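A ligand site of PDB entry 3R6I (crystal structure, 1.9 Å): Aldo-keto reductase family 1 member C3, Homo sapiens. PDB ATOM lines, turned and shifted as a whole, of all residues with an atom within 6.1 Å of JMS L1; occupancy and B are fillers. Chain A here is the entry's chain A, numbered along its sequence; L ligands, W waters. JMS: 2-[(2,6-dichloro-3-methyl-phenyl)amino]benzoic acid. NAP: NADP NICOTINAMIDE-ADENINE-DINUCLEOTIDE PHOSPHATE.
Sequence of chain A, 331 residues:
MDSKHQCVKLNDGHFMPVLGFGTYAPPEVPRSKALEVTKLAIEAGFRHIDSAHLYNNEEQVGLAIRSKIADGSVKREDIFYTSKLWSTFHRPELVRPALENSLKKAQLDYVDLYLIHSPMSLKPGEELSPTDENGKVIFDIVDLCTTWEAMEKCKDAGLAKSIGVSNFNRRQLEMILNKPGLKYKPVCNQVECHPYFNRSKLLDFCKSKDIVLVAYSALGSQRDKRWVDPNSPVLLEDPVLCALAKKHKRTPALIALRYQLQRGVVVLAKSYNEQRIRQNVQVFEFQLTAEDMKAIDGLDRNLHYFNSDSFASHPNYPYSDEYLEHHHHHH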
ATOM      1  N   TYR A  24       7.088 -10.362  28.613  1.00  0.00           N
ATOM      2  CA  TYR A  24       7.950  -9.213  28.914  1.00  0.00           C
ATOM      3  C   TYR A  24       8.622  -9.379  30.305  1.00  0.00           C
ATOM      4  O   TYR A  24       7.945  -9.722  31.291  1.00  0.00           O
ATOM      5  CB  TYR A  24       7.199  -7.868  28.880  1.00  0.00           C
ATOM      6  CG  TYR A  24       8.140  -6.741  29.263  1.00  0.00           C
ATOM      7  CD1 TYR A  24       9.080  -6.270  28.339  1.00  0.00           C
ATOM      8  CD2 TYR A  24       8.147  -6.178  30.569  1.00  0.00           C
ATOM      9  CE1 TYR A  24      10.012  -5.248  28.652  1.00  0.00           C
ATOM     10  CE2 TYR A  24       9.065  -5.161  30.923  1.00  0.00           C
ATOM     11  CZ  TYR A  24       9.998  -4.707  29.930  1.00  0.00           C
ATOM     12  OH  TYR A  24      10.891  -3.710  30.161  1.00  0.00           O
ATOM     13  N   ALA A  52       7.000  -9.237  21.454  1.00  0.00           N
ATOM     14  CA  ALA A  52       7.037  -7.924  20.750  1.00  0.00           C
ATOM     15  C   ALA A  52       8.480  -7.641  20.399  1.00  0.00           C
ATOM     16  O   ALA A  52       9.370  -8.116  21.112  1.00  0.00           O
ATOM     17  CB  ALA A  52       6.519  -6.743  21.688  1.00  0.00           C
ATOM     18  N   LEU A  54       9.773  -4.800  20.889  1.00  0.00           N
ATOM     19  CA  LEU A  54      10.177  -4.083  22.135  1.00  0.00           C
ATOM     20  C   LEU A  54      10.814  -4.928  23.234  1.00  0.00           C
ATOM     21  O   LEU A  54      11.730  -4.464  23.964  1.00  0.00           O
ATOM     22  CB  LEU A  54       8.972  -3.360  22.740  1.00  0.00           C
ATOM     23  CG  LEU A  54       9.233  -2.372  23.922  1.00  0.00           C
ATOM     24  CD1 LEU A  54      10.141  -1.130  23.575  1.00  0.00           C
ATOM     25  CD2 LEU A  54       7.894  -1.895  24.522  1.00  0.00           C
ATOM     26  N   TYR A  55      10.337  -6.155  23.389  1.00  0.00           N
ATOM     27  CA  TYR A  55      10.748  -7.008  24.545  1.00  0.00           C
ATOM     28  C   TYR A  55      12.177  -7.558  24.538  1.00  0.00           C
ATOM     29  O   TYR A  55      12.645  -8.069  25.575  1.00  0.00           O
ATOM     30  CB  TYR A  55       9.761  -8.158  24.777  1.00  0.00           C
ATOM     31  CG  TYR A  55       8.292  -7.677  24.899  1.00  0.00           C
ATOM     32  CD1 TYR A  55       7.994  -6.306  25.092  1.00  0.00           C
ATOM     33  CD2 TYR A  55       7.238  -8.614  24.862  1.00  0.00           C
ATOM     34  CE1 TYR A  55       6.633  -5.851  25.232  1.00  0.00           C
ATOM     35  CE2 TYR A  55       5.861  -8.204  24.939  1.00  0.00           C
ATOM     36  CZ  TYR A  55       5.580  -6.813  25.147  1.00  0.00           C
ATOM     37  OH  TYR A  55       4.273  -6.361  25.232  1.00  0.00           O
ATOM     38  N   LYS A  84       4.605  -7.736  17.773  1.00  0.00           N
ATOM     39  CA  LYS A  84       4.065  -6.357  17.724  1.00  0.00           C
ATOM     40  C   LYS A  84       5.043  -5.449  17.050  1.00  0.00           C
ATOM     41  O   LYS A  84       6.244  -5.451  17.319  1.00  0.00           O
ATOM     42  CB  LYS A  84       3.709  -5.785  19.093  1.00  0.00           C
ATOM     43  CG  LYS A  84       2.923  -6.755  20.035  1.00  0.00           C
ATOM     44  CD  LYS A  84       2.491  -5.970  21.305  1.00  0.00           C
ATOM     45  CE  LYS A  84       1.834  -7.043  22.302  1.00  0.00           C
ATOM     46  NZ  LYS A  84       2.851  -7.746  23.120  1.00  0.00           N
ATOM     47  N   TRP A  86       6.892  -2.139  16.538  1.00  0.00           N
ATOM     48  CA  TRP A  86       7.305  -1.058  17.394  1.00  0.00           C
ATOM     49  C   TRP A  86       7.005   0.315  16.738  1.00  0.00           C
ATOM     50  O   TRP A  86       6.889   0.436  15.498  1.00  0.00           O
ATOM     51  CB  TRP A  86       8.771  -1.199  17.854  1.00  0.00           C
ATOM     52  CG  TRP A  86       9.112  -0.097  18.840  1.00  0.00           C
ATOM     53  CD1 TRP A  86      10.125   0.838  18.725  1.00  0.00           C
ATOM     54  CD2 TRP A  86       8.363   0.244  20.008  1.00  0.00           C
ATOM     55  NE1 TRP A  86      10.061   1.721  19.804  1.00  0.00           N
ATOM     56  CE2 TRP A  86       8.980   1.397  20.589  1.00  0.00           C
ATOM     57  CE3 TRP A  86       7.216  -0.295  20.615  1.00  0.00           C
ATOM     58  CZ2 TRP A  86       8.500   2.012  21.779  1.00  0.00           C
ATOM     59  CZ3 TRP A  86       6.728   0.327  21.784  1.00  0.00           C
ATOM     60  CH2 TRP A  86       7.376   1.476  22.336  1.00  0.00           C
ATOM     61  N   SER A  87       6.890   1.349  17.554  1.00  0.00           N
ATOM     62  CA  SER A  87       6.317   2.654  17.202  1.00  0.00           C
ATOM     63  C   SER A  87       7.238   3.544  16.339  1.00  0.00           C
ATOM     64  O   SER A  87       6.773   4.568  15.768  1.00  0.00           O
ATOM     65  CB  SER A  87       6.025   3.401  18.529  1.00  0.00           C
ATOM     66  OG  SER A  87       5.110   2.588  19.247  1.00  0.00           O
ATOM     67  N   HIS A 117       1.806  -1.915  18.040  1.00  0.00           N
ATOM     68  CA  HIS A 117       2.071  -2.015  19.509  1.00  0.00           C
ATOM     69  C   HIS A 117       1.373  -0.821  20.168  1.00  0.00           C
ATOM     70  O   HIS A 117       0.867  -0.908  21.325  1.00  0.00           O
ATOM     71  CB  HIS A 117       3.611  -2.004  19.826  1.00  0.00           C
ATOM     72  CG  HIS A 117       3.968  -2.569  21.173  1.00  0.00           C
ATOM     73  ND1 HIS A 117       5.136  -3.263  21.400  1.00  0.00           N
ATOM     74  CD2 HIS A 117       3.332  -2.484  22.381  1.00  0.00           C
ATOM     75  CE1 HIS A 117       5.168  -3.666  22.667  1.00  0.00           C
ATOM     76  NE2 HIS A 117       4.113  -3.165  23.304  1.00  0.00           N
ATOM     77  N   SER A 118       1.368   0.332  19.484  1.00  0.00           N
ATOM     78  CA  SER A 118       0.896   1.538  20.181  1.00  0.00           C
ATOM     79  C   SER A 118       0.520   2.543  19.126  1.00  0.00           C
ATOM     80  O   SER A 118       1.164   2.554  18.040  1.00  0.00           O
ATOM     81  CB  SER A 118       2.047   2.057  21.101  1.00  0.00           C
ATOM     82  OG  SER A 118       1.983   3.450  21.328  1.00  0.00           O
ATOM     83  N   MET A 120       1.120   5.637  19.416  1.00  0.00           N
ATOM     84  CA  MET A 120       1.949   6.813  19.559  1.00  0.00           C
ATOM     85  C   MET A 120       3.186   6.699  18.709  1.00  0.00           C
ATOM     86  O   MET A 120       4.209   6.184  19.172  1.00  0.00           O
ATOM     87  CB  MET A 120       2.342   7.023  20.993  1.00  0.00           C
ATOM     88  CG  MET A 120       1.136   7.390  21.889  1.00  0.00           C
ATOM     89  SD  MET A 120       1.482   7.424  23.684  1.00  0.00           S
ATOM     90  CE  MET A 120       1.687   5.644  24.032  1.00  0.00           C
ATOM     91  N   ASN A 167      -3.262  -0.797  22.595  1.00  0.00           N
ATOM     92  CA  ASN A 167      -3.251   0.528  23.227  1.00  0.00           C
ATOM     93  C   ASN A 167      -4.076   1.583  22.450  1.00  0.00           C
ATOM     94  O   ASN A 167      -3.816   2.803  22.577  1.00  0.00           O
ATOM     95  CB  ASN A 167      -1.812   1.019  23.437  1.00  0.00           C
ATOM     96  CG  ASN A 167      -1.087   0.242  24.527  1.00  0.00           C
ATOM     97  OD1 ASN A 167      -1.578   0.143  25.682  1.00  0.00           O
ATOM     98  ND2 ASN A 167       0.021  -0.389  24.163  1.00  0.00           N
ATOM     99  N   GLN A 190      -5.372  -4.960  22.181  1.00  0.00           N
ATOM    100  CA  GLN A 190      -4.763  -5.410  23.441  1.00  0.00           C
ATOM    101  C   GLN A 190      -4.502  -4.182  24.306  1.00  0.00           C
ATOM    102  O   GLN A 190      -3.788  -3.257  23.877  1.00  0.00           O
ATOM    103  CB  GLN A 190      -3.460  -6.196  23.170  1.00  0.00           C
ATOM    104  CG  GLN A 190      -2.754  -6.639  24.474  1.00  0.00           C
ATOM    105  CD  GLN A 190      -1.455  -7.374  24.159  1.00  0.00           C
ATOM    106  OE1 GLN A 190      -0.399  -6.947  24.806  1.00  0.00           O
ATOM    107  NE2 GLN A 190      -1.405  -8.323  23.321  1.00  0.00           N
ATOM    108  N   GLU A 192      -4.508  -2.180  28.531  1.00  0.00           N
ATOM    109  CA  GLU A 192      -4.405  -2.323  29.953  1.00  0.00           C
ATOM    110  C   GLU A 192      -5.799  -2.615  30.500  1.00  0.00           C
ATOM    111  O   GLU A 192      -6.714  -1.895  30.222  1.00  0.00           O
ATOM    112  CB  GLU A 192      -3.768  -1.108  30.666  1.00  0.00           C
ATOM    113  CG  GLU A 192      -3.531  -1.513  32.131  1.00  0.00           C
ATOM    114  CD  GLU A 192      -2.794  -0.439  33.020  1.00  0.00           C
ATOM    115  OE1 GLU A 192      -1.945   0.349  32.467  1.00  0.00           O
ATOM    116  OE2 GLU A 192      -3.081  -0.365  34.301  1.00  0.00           O
ATOM    117  N   TYR A 216      -3.860  -6.762  29.091  1.00  0.00           N
ATOM    118  CA  TYR A 216      -2.535  -6.863  29.730  1.00  0.00           C
ATOM    119  C   TYR A 216      -2.495  -6.196  31.100  1.00  0.00           C
ATOM    120  O   TYR A 216      -3.398  -5.452  31.430  1.00  0.00           O
ATOM    121  CB  TYR A 216      -1.413  -6.333  28.808  1.00  0.00           C
ATOM    122  CG  TYR A 216      -1.379  -4.836  28.594  1.00  0.00           C
ATOM    123  CD1 TYR A 216      -1.064  -3.977  29.632  1.00  0.00           C
ATOM    124  CD2 TYR A 216      -1.605  -4.292  27.331  1.00  0.00           C
ATOM    125  CE1 TYR A 216      -0.958  -2.618  29.425  1.00  0.00           C
ATOM    126  CE2 TYR A 216      -1.483  -2.894  27.114  1.00  0.00           C
ATOM    127  CZ  TYR A 216      -1.168  -2.104  28.163  1.00  0.00           C
ATOM    128  OH  TYR A 216      -1.040  -0.736  27.979  1.00  0.00           O
ATOM    129  N   SER A 217      -1.459  -6.520  31.910  1.00  0.00           N
ATOM    130  CA  SER A 217      -1.414  -6.084  33.302  1.00  0.00           C
ATOM    131  C   SER A 217      -2.684  -6.500  34.017  1.00  0.00           C
ATOM    132  O   SER A 217      -3.157  -5.803  34.893  1.00  0.00           O
ATOM    133  CB  SER A 217      -1.147  -4.543  33.492  1.00  0.00           C
ATOM    134  OG  SER A 217       0.046  -4.182  32.794  1.00  0.00           O
ATOM    135  N   ARG A 226      10.046   2.680  36.382  1.00  0.00           N
ATOM    136  CA  ARG A 226      10.163   3.526  35.179  1.00  0.00           C
ATOM    137  C   ARG A 226       8.813   4.077  34.685  1.00  0.00           C
ATOM    138  O   ARG A 226       8.791   5.145  34.092  1.00  0.00           O
ATOM    139  CB  ARG A 226      10.820   2.723  34.047  1.00  0.00           C
ATOM    140  CG  ARG A 226      12.354   2.411  34.322  1.00  0.00           C
ATOM    141  CD  ARG A 226      13.000   1.626  33.197  1.00  0.00           C
ATOM    142  NE  ARG A 226      12.567   0.238  33.223  1.00  0.00           N
ATOM    143  CZ  ARG A 226      12.624  -0.575  32.178  1.00  0.00           C
ATOM    144  NH1 ARG A 226      13.133  -0.145  31.002  1.00  0.00           N
ATOM    145  NH2 ARG A 226      12.174  -1.829  32.303  1.00  0.00           N
ATOM    146  N   TRP A 227       7.690   3.383  34.916  1.00  0.00           N
ATOM    147  CA  TRP A 227       6.384   3.934  34.494  1.00  0.00           C
ATOM    148  C   TRP A 227       5.299   3.837  35.557  1.00  0.00           C
ATOM    149  O   TRP A 227       4.249   4.430  35.395  1.00  0.00           O
ATOM    150  CB  TRP A 227       5.857   3.294  33.181  1.00  0.00           C
ATOM    151  CG  TRP A 227       6.921   3.156  32.153  1.00  0.00           C
ATOM    152  CD1 TRP A 227       7.399   4.137  31.312  1.00  0.00           C
ATOM    153  CD2 TRP A 227       7.721   2.010  31.932  1.00  0.00           C
ATOM    154  NE1 TRP A 227       8.457   3.654  30.568  1.00  0.00           N
ATOM    155  CE2 TRP A 227       8.651   2.343  30.922  1.00  0.00           C
ATOM    156  CE3 TRP A 227       7.717   0.712  32.480  1.00  0.00           C
ATOM    157  CZ2 TRP A 227       9.563   1.447  30.445  1.00  0.00           C
ATOM    158  CZ3 TRP A 227       8.638  -0.172  32.000  1.00  0.00           C
ATOM    159  CH2 TRP A 227       9.547   0.199  31.003  1.00  0.00           C
ATOM    160  N   PHE A 306       0.442   2.199  34.090  1.00  0.00           N
ATOM    161  CA  PHE A 306       1.482   2.887  33.284  1.00  0.00           C
ATOM    162  C   PHE A 306       1.108   4.334  33.262  1.00  0.00           C
ATOM    163  O   PHE A 306       0.082   4.658  32.699  1.00  0.00           O
ATOM    164  CB  PHE A 306       1.599   2.319  31.872  1.00  0.00           C
ATOM    165  CG  PHE A 306       2.128   0.927  31.910  1.00  0.00           C
ATOM    166  CD1 PHE A 306       3.537   0.678  31.705  1.00  0.00           C
ATOM    167  CD2 PHE A 306       1.280  -0.156  32.299  1.00  0.00           C
ATOM    168  CE1 PHE A 306       4.081  -0.636  31.822  1.00  0.00           C
ATOM    169  CE2 PHE A 306       1.789  -1.502  32.437  1.00  0.00           C
ATOM    170  CZ  PHE A 306       3.195  -1.752  32.195  1.00  0.00           C
ATOM    171  N   PHE A 311       4.578   8.989  28.020  1.00  0.00           N
ATOM    172  CA  PHE A 311       3.439   8.700  27.142  1.00  0.00           C
ATOM    173  C   PHE A 311       2.539   9.908  27.133  1.00  0.00           C
ATOM    174  O   PHE A 311       2.049  10.289  26.093  1.00  0.00           O
ATOM    175  CB  PHE A 311       2.607   7.518  27.682  1.00  0.00           C
ATOM    176  CG  PHE A 311       3.416   6.241  27.920  1.00  0.00           C
ATOM    177  CD1 PHE A 311       4.330   5.764  26.928  1.00  0.00           C
ATOM    178  CD2 PHE A 311       3.246   5.505  29.153  1.00  0.00           C
ATOM    179  CE1 PHE A 311       5.059   4.544  27.195  1.00  0.00           C
ATOM    180  CE2 PHE A 311       3.970   4.293  29.434  1.00  0.00           C
ATOM    181  CZ  PHE A 311       4.885   3.829  28.484  1.00  0.00           C
ATOM    182  N   TYR A 317      -1.430  10.001  22.702  1.00  0.00           N
ATOM    183  CA  TYR A 317      -1.668   9.333  23.997  1.00  0.00           C
ATOM    184  C   TYR A 317      -3.088   8.765  24.066  1.00  0.00           C
ATOM    185  O   TYR A 317      -4.036   9.515  24.003  1.00  0.00           O
ATOM    186  CB  TYR A 317      -1.545  10.384  25.067  1.00  0.00           C
ATOM    187  CG  TYR A 317      -1.565   9.831  26.450  1.00  0.00           C
ATOM    188  CD1 TYR A 317      -0.718   8.773  26.812  1.00  0.00           C
ATOM    189  CD2 TYR A 317      -2.359  10.421  27.420  1.00  0.00           C
ATOM    190  CE1 TYR A 317      -0.698   8.275  28.178  1.00  0.00           C
ATOM    191  CE2 TYR A 317      -2.369   9.919  28.763  1.00  0.00           C
ATOM    192  CZ  TYR A 317      -1.533   8.865  29.112  1.00  0.00           C
ATOM    193  OH  TYR A 317      -1.527   8.422  30.421  1.00  0.00           O
ATOM    194  N   PRO A 318      -3.224   7.452  24.265  1.00  0.00           N
ATOM    195  CA  PRO A 318      -4.557   6.910  24.246  1.00  0.00           C
ATOM    196  C   PRO A 318      -5.399   7.293  25.420  1.00  0.00           C
ATOM    197  O   PRO A 318      -6.615   7.224  25.284  1.00  0.00           O
ATOM    198  CB  PRO A 318      -4.337   5.398  24.224  1.00  0.00           C
ATOM    199  CG  PRO A 318      -3.004   5.218  24.917  1.00  0.00           C
ATOM    200  CD  PRO A 318      -2.199   6.401  24.346  1.00  0.00           C
ATOM    201  N   TYR A 319      -4.814   7.716  26.544  1.00  0.00           N
ATOM    202  CA  TYR A 319      -5.673   8.015  27.669  1.00  0.00           C
ATOM    203  C   TYR A 319      -6.052   9.508  27.751  1.00  0.00           C
ATOM    204  O   TYR A 319      -6.602   9.929  28.797  1.00  0.00           O
ATOM    205  CB  TYR A 319      -5.073   7.560  29.006  1.00  0.00           C
ATOM    206  CG  TYR A 319      -4.668   6.106  29.022  1.00  0.00           C
ATOM    207  CD1 TYR A 319      -5.573   5.109  28.647  1.00  0.00           C
ATOM    208  CD2 TYR A 319      -3.407   5.749  29.416  1.00  0.00           C
ATOM    209  CE1 TYR A 319      -5.189   3.690  28.699  1.00  0.00           C
ATOM    210  CE2 TYR A 319      -3.025   4.377  29.468  1.00  0.00           C
ATOM    211  CZ  TYR A 319      -3.941   3.365  29.105  1.00  0.00           C
ATOM    212  OH  TYR A 319      -3.543   2.032  29.148  1.00  0.00           O
HETATM  213  OXT JMS L   1       4.871  -5.001  27.812  1.00  0.00           O
HETATM  214  C7  JMS L   1       4.857  -3.975  27.106  1.00  0.00           C
HETATM  215  OH  JMS L   1       4.439  -3.986  25.953  1.00  0.00           O
HETATM  216  C1  JMS L   1       5.519  -2.744  27.693  1.00  0.00           C
HETATM  217  C6  JMS L   1       6.631  -2.988  28.533  1.00  0.00           C
HETATM  218  C5  JMS L   1       7.307  -1.913  29.172  1.00  0.00           C
HETATM  219  C4  JMS L   1       6.818  -0.597  28.954  1.00  0.00           C
HETATM  220  C3  JMS L   1       5.677  -0.362  28.137  1.00  0.00           C
HETATM  221  C2  JMS L   1       5.027  -1.448  27.465  1.00  0.00           C
HETATM  222  N   JMS L   1       3.911  -1.203  26.707  1.00  0.00           N
HETATM  223  C1B JMS L   1       3.258   0.024  26.524  1.00  0.00           C
HETATM  224  C2B JMS L   1       2.377   0.659  27.410  1.00  0.00           C
HETATM  225 CL1  JMS L   1       2.170  -0.146  28.933  1.00  0.00          CL
HETATM  226  C3B JMS L   1       1.784   1.893  27.015  1.00  0.00           C
HETATM  227  C7B JMS L   1       0.834   2.788  27.771  1.00  0.00           C
HETATM  228  C4B JMS L   1       2.013   2.487  25.807  1.00  0.00           C
HETATM  229  C5B JMS L   1       2.863   1.908  24.941  1.00  0.00           C
HETATM  230  C6B JMS L   1       3.399   0.684  25.324  1.00  0.00           C
HETATM  231 CL2  JMS L   1       4.434   0.050  24.193  1.00  0.00          CL
HETATM  232  PA  NAP L   2       0.962  -9.193  34.677  1.00  0.00           P
HETATM  233  O1A NAP L   2       0.291 -10.241  33.879  1.00  0.00           O
HETATM  234  O2A NAP L   2       0.086  -8.054  35.209  1.00  0.00           O
HETATM  235  O5B NAP L   2       1.738  -9.748  36.013  1.00  0.00           O
HETATM  236  C5B NAP L   2       2.239  -8.883  36.981  1.00  0.00           C
HETATM  237  C4B NAP L   2       3.028  -9.724  38.067  1.00  0.00           C
HETATM  238  O4B NAP L   2       2.102 -10.741  38.433  1.00  0.00           O
HETATM  239  C3B NAP L   2       4.054 -10.538  37.341  1.00  0.00           C
HETATM  240  O3B NAP L   2       5.239  -9.820  37.327  1.00  0.00           O
HETATM  241  C2B NAP L   2       4.157 -11.844  38.160  1.00  0.00           C
HETATM  242  O2B NAP L   2       5.355 -11.920  38.983  1.00  0.00           O
HETATM  243  C1B NAP L   2       2.977 -11.757  39.024  1.00  0.00           C
HETATM  244  N9A NAP L   2       2.181 -13.051  38.981  1.00  0.00           N
HETATM  245  C8A NAP L   2       1.893 -13.854  37.921  1.00  0.00           C
HETATM  246  N7A NAP L   2       1.107 -14.839  38.310  1.00  0.00           N
HETATM  247  C5A NAP L   2       0.882 -14.668  39.612  1.00  0.00           C
HETATM  248  C6A NAP L   2       0.233 -15.456  40.562  1.00  0.00           C
HETATM  249  N6A NAP L   2      -0.429 -16.583  40.214  1.00  0.00           N
HETATM  250  N1A NAP L   2       0.236 -15.011  41.829  1.00  0.00           N
HETATM  251  C2A NAP L   2       0.883 -13.859  42.220  1.00  0.00           C
HETATM  252  N3A NAP L   2       1.565 -13.121  41.360  1.00  0.00           N
HETATM  253  C4A NAP L   2       1.587 -13.531  40.059  1.00  0.00           C
HETATM  254  O3  NAP L   2       2.178  -8.435  33.867  1.00  0.00           O
HETATM  255  PN  NAP L   2       2.397  -7.466  32.629  1.00  0.00           P
HETATM  256  O1N NAP L   2       3.781  -7.810  32.239  1.00  0.00           O
HETATM  257  O2N NAP L   2       1.966  -6.059  32.977  1.00  0.00           O
HETATM  258  O5D NAP L   2       1.291  -8.007  31.571  1.00  0.00           O
HETATM  259  C5D NAP L   2       1.470  -9.381  30.958  1.00  0.00           C
HETATM  260  C4D NAP L   2       1.921  -9.368  29.525  1.00  0.00           C
HETATM  261  O4D NAP L   2       1.083  -8.455  28.811  1.00  0.00           O
HETATM  262  C3D NAP L   2       3.317  -8.715  29.330  1.00  0.00           C
HETATM  263  O3D NAP L   2       4.305  -9.651  29.832  1.00  0.00           O
HETATM  264  C2D NAP L   2       3.314  -8.544  27.823  1.00  0.00           C
HETATM  265  O2D NAP L   2       3.338  -9.842  27.215  1.00  0.00           O
HETATM  266  C1D NAP L   2       1.857  -7.956  27.632  1.00  0.00           C
HETATM  267  N1N NAP L   2       1.841  -6.478  27.835  1.00  0.00           N
HETATM  268  C2N NAP L   2       1.639  -5.748  26.676  1.00  0.00           C
HETATM  269  C3N NAP L   2       1.596  -4.342  26.764  1.00  0.00           C
HETATM  270  C7N NAP L   2       1.324  -3.555  25.487  1.00  0.00           C
HETATM  271  O7N NAP L   2       1.670  -2.357  25.371  1.00  0.00           O
HETATM  272  N7N NAP L   2       0.516  -4.202  24.565  1.00  0.00           N
HETATM  273  C4N NAP L   2       1.831  -3.715  27.996  1.00  0.00           C
HETATM  274  C5N NAP L   2       2.037  -4.494  29.177  1.00  0.00           C
HETATM  275  C6N NAP L   2       2.061  -5.893  29.099  1.00  0.00           C
HETATM  276  P2B NAP L   2       6.326 -13.295  38.799  1.00  0.00           P
HETATM  277  O1X NAP L   2       6.964 -13.223  37.440  1.00  0.00           O
HETATM  278  O2X NAP L   2       7.275 -13.184  40.019  1.00  0.00           O
HETATM  279  O3X NAP L   2       5.323 -14.473  38.965  1.00  0.00           O
HETATM  280  O   HOH W   1       5.033  -5.172  30.610  1.00  0.00           O
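The side-chain hydroxyl (OH) of Tyr 55 sits at hydrogen-bond distance from an oxygen (OH) of JMS L1 (2.5 Å). A ring nitrogen (NE2) of His 117 lies within hydrogen-bond range of an oxygen (OH) of JMS L1 (2.8 Å). A ring nitrogen (NE2) of His 117 lies within hydrogen-bond range of an oxygen (O7N) of NAP L2, at 3.3 Å. O7N of NAP L2 is in hydrogen-bond range of ND2 of Asn 167 (2.8 Å). The backbone NH (N) of Tyr 24 sits at hydrogen-bond distance from an oxygen (O3D) of NAP L2 (3.1 Å). The side-chain amide oxygen (OE1) of Gln 190 sits at hydrogen-bond distance from a nitrogen (N7N) of NAP L2 (2.9 Å). N of Ser 217 is in hydrogen-bond range of O5D of NAP L2. The side-chain hydroxyl of Ser 217 lies within hydrogen-bond range of an oxygen (O2N) of NAP L2.
N of JMS L1 sits at hydrogen-bond distance from O7N of NAP L2, 2.9 Å away.
OH of Tyr 55 is in hydrogen-bond range of NZ of Lys 84. The backbone carbonyl oxygen (O) of His 117 sits at hydrogen-bond distance from the side-chain amide nitrogen (ND2) of Asn 167, 3.0 Å away. The backbone NH (N) of Phe 306 lies close to the side-chain carboxylate (OE1) of Glu 192 (3.4 Å). The side-chain amide oxygen (OD1) of Asn 167 sits at hydrogen-bond distance from the side-chain hydroxyl (OH) of Tyr 216 (2.5 Å). OG of Ser 118 sits at hydrogen-bond distance from N of Met 120, 3.0 Å away. The backbone carbonyl oxygen of Gln 190 lies within hydrogen-bond range of the backbone NH of Asn 167 (2.8 Å). OH of Tyr 24 lies within hydrogen-bond range of NH2 of Arg 226, 3.1 Å away.
Merely in contact with JMS L1: Phe 306 (3.2 Å), Trp 86 (3.3 Å), Tyr 216 (3.4 Å), Trp 227 (3.5 Å), Met 120 (3.6 Å), Asn 167 (3.7 Å), Tyr 24 (3.8 Å), Phe 311 (3.9 Å), Ser 118 (3.9 Å) and Leu 54 (3.98 Å). Hydrophobic or aromatic side chains within 4 Å of JMS L1: Tyr 24, Leu 54, Tyr 55, Trp 86, His 117, Met 120, Tyr 216, Trp 227, Phe 306 and Phe 311. The nearest printed residue that does not touch JMS L1 is Tyr 319 (4.5 Å).
Water W1 lies within hydrogen-bond range of an oxygen (OXT) of JMS L1 (2.8 Å) and an oxygen (O1N) of NAP L2 (3.3 Å).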
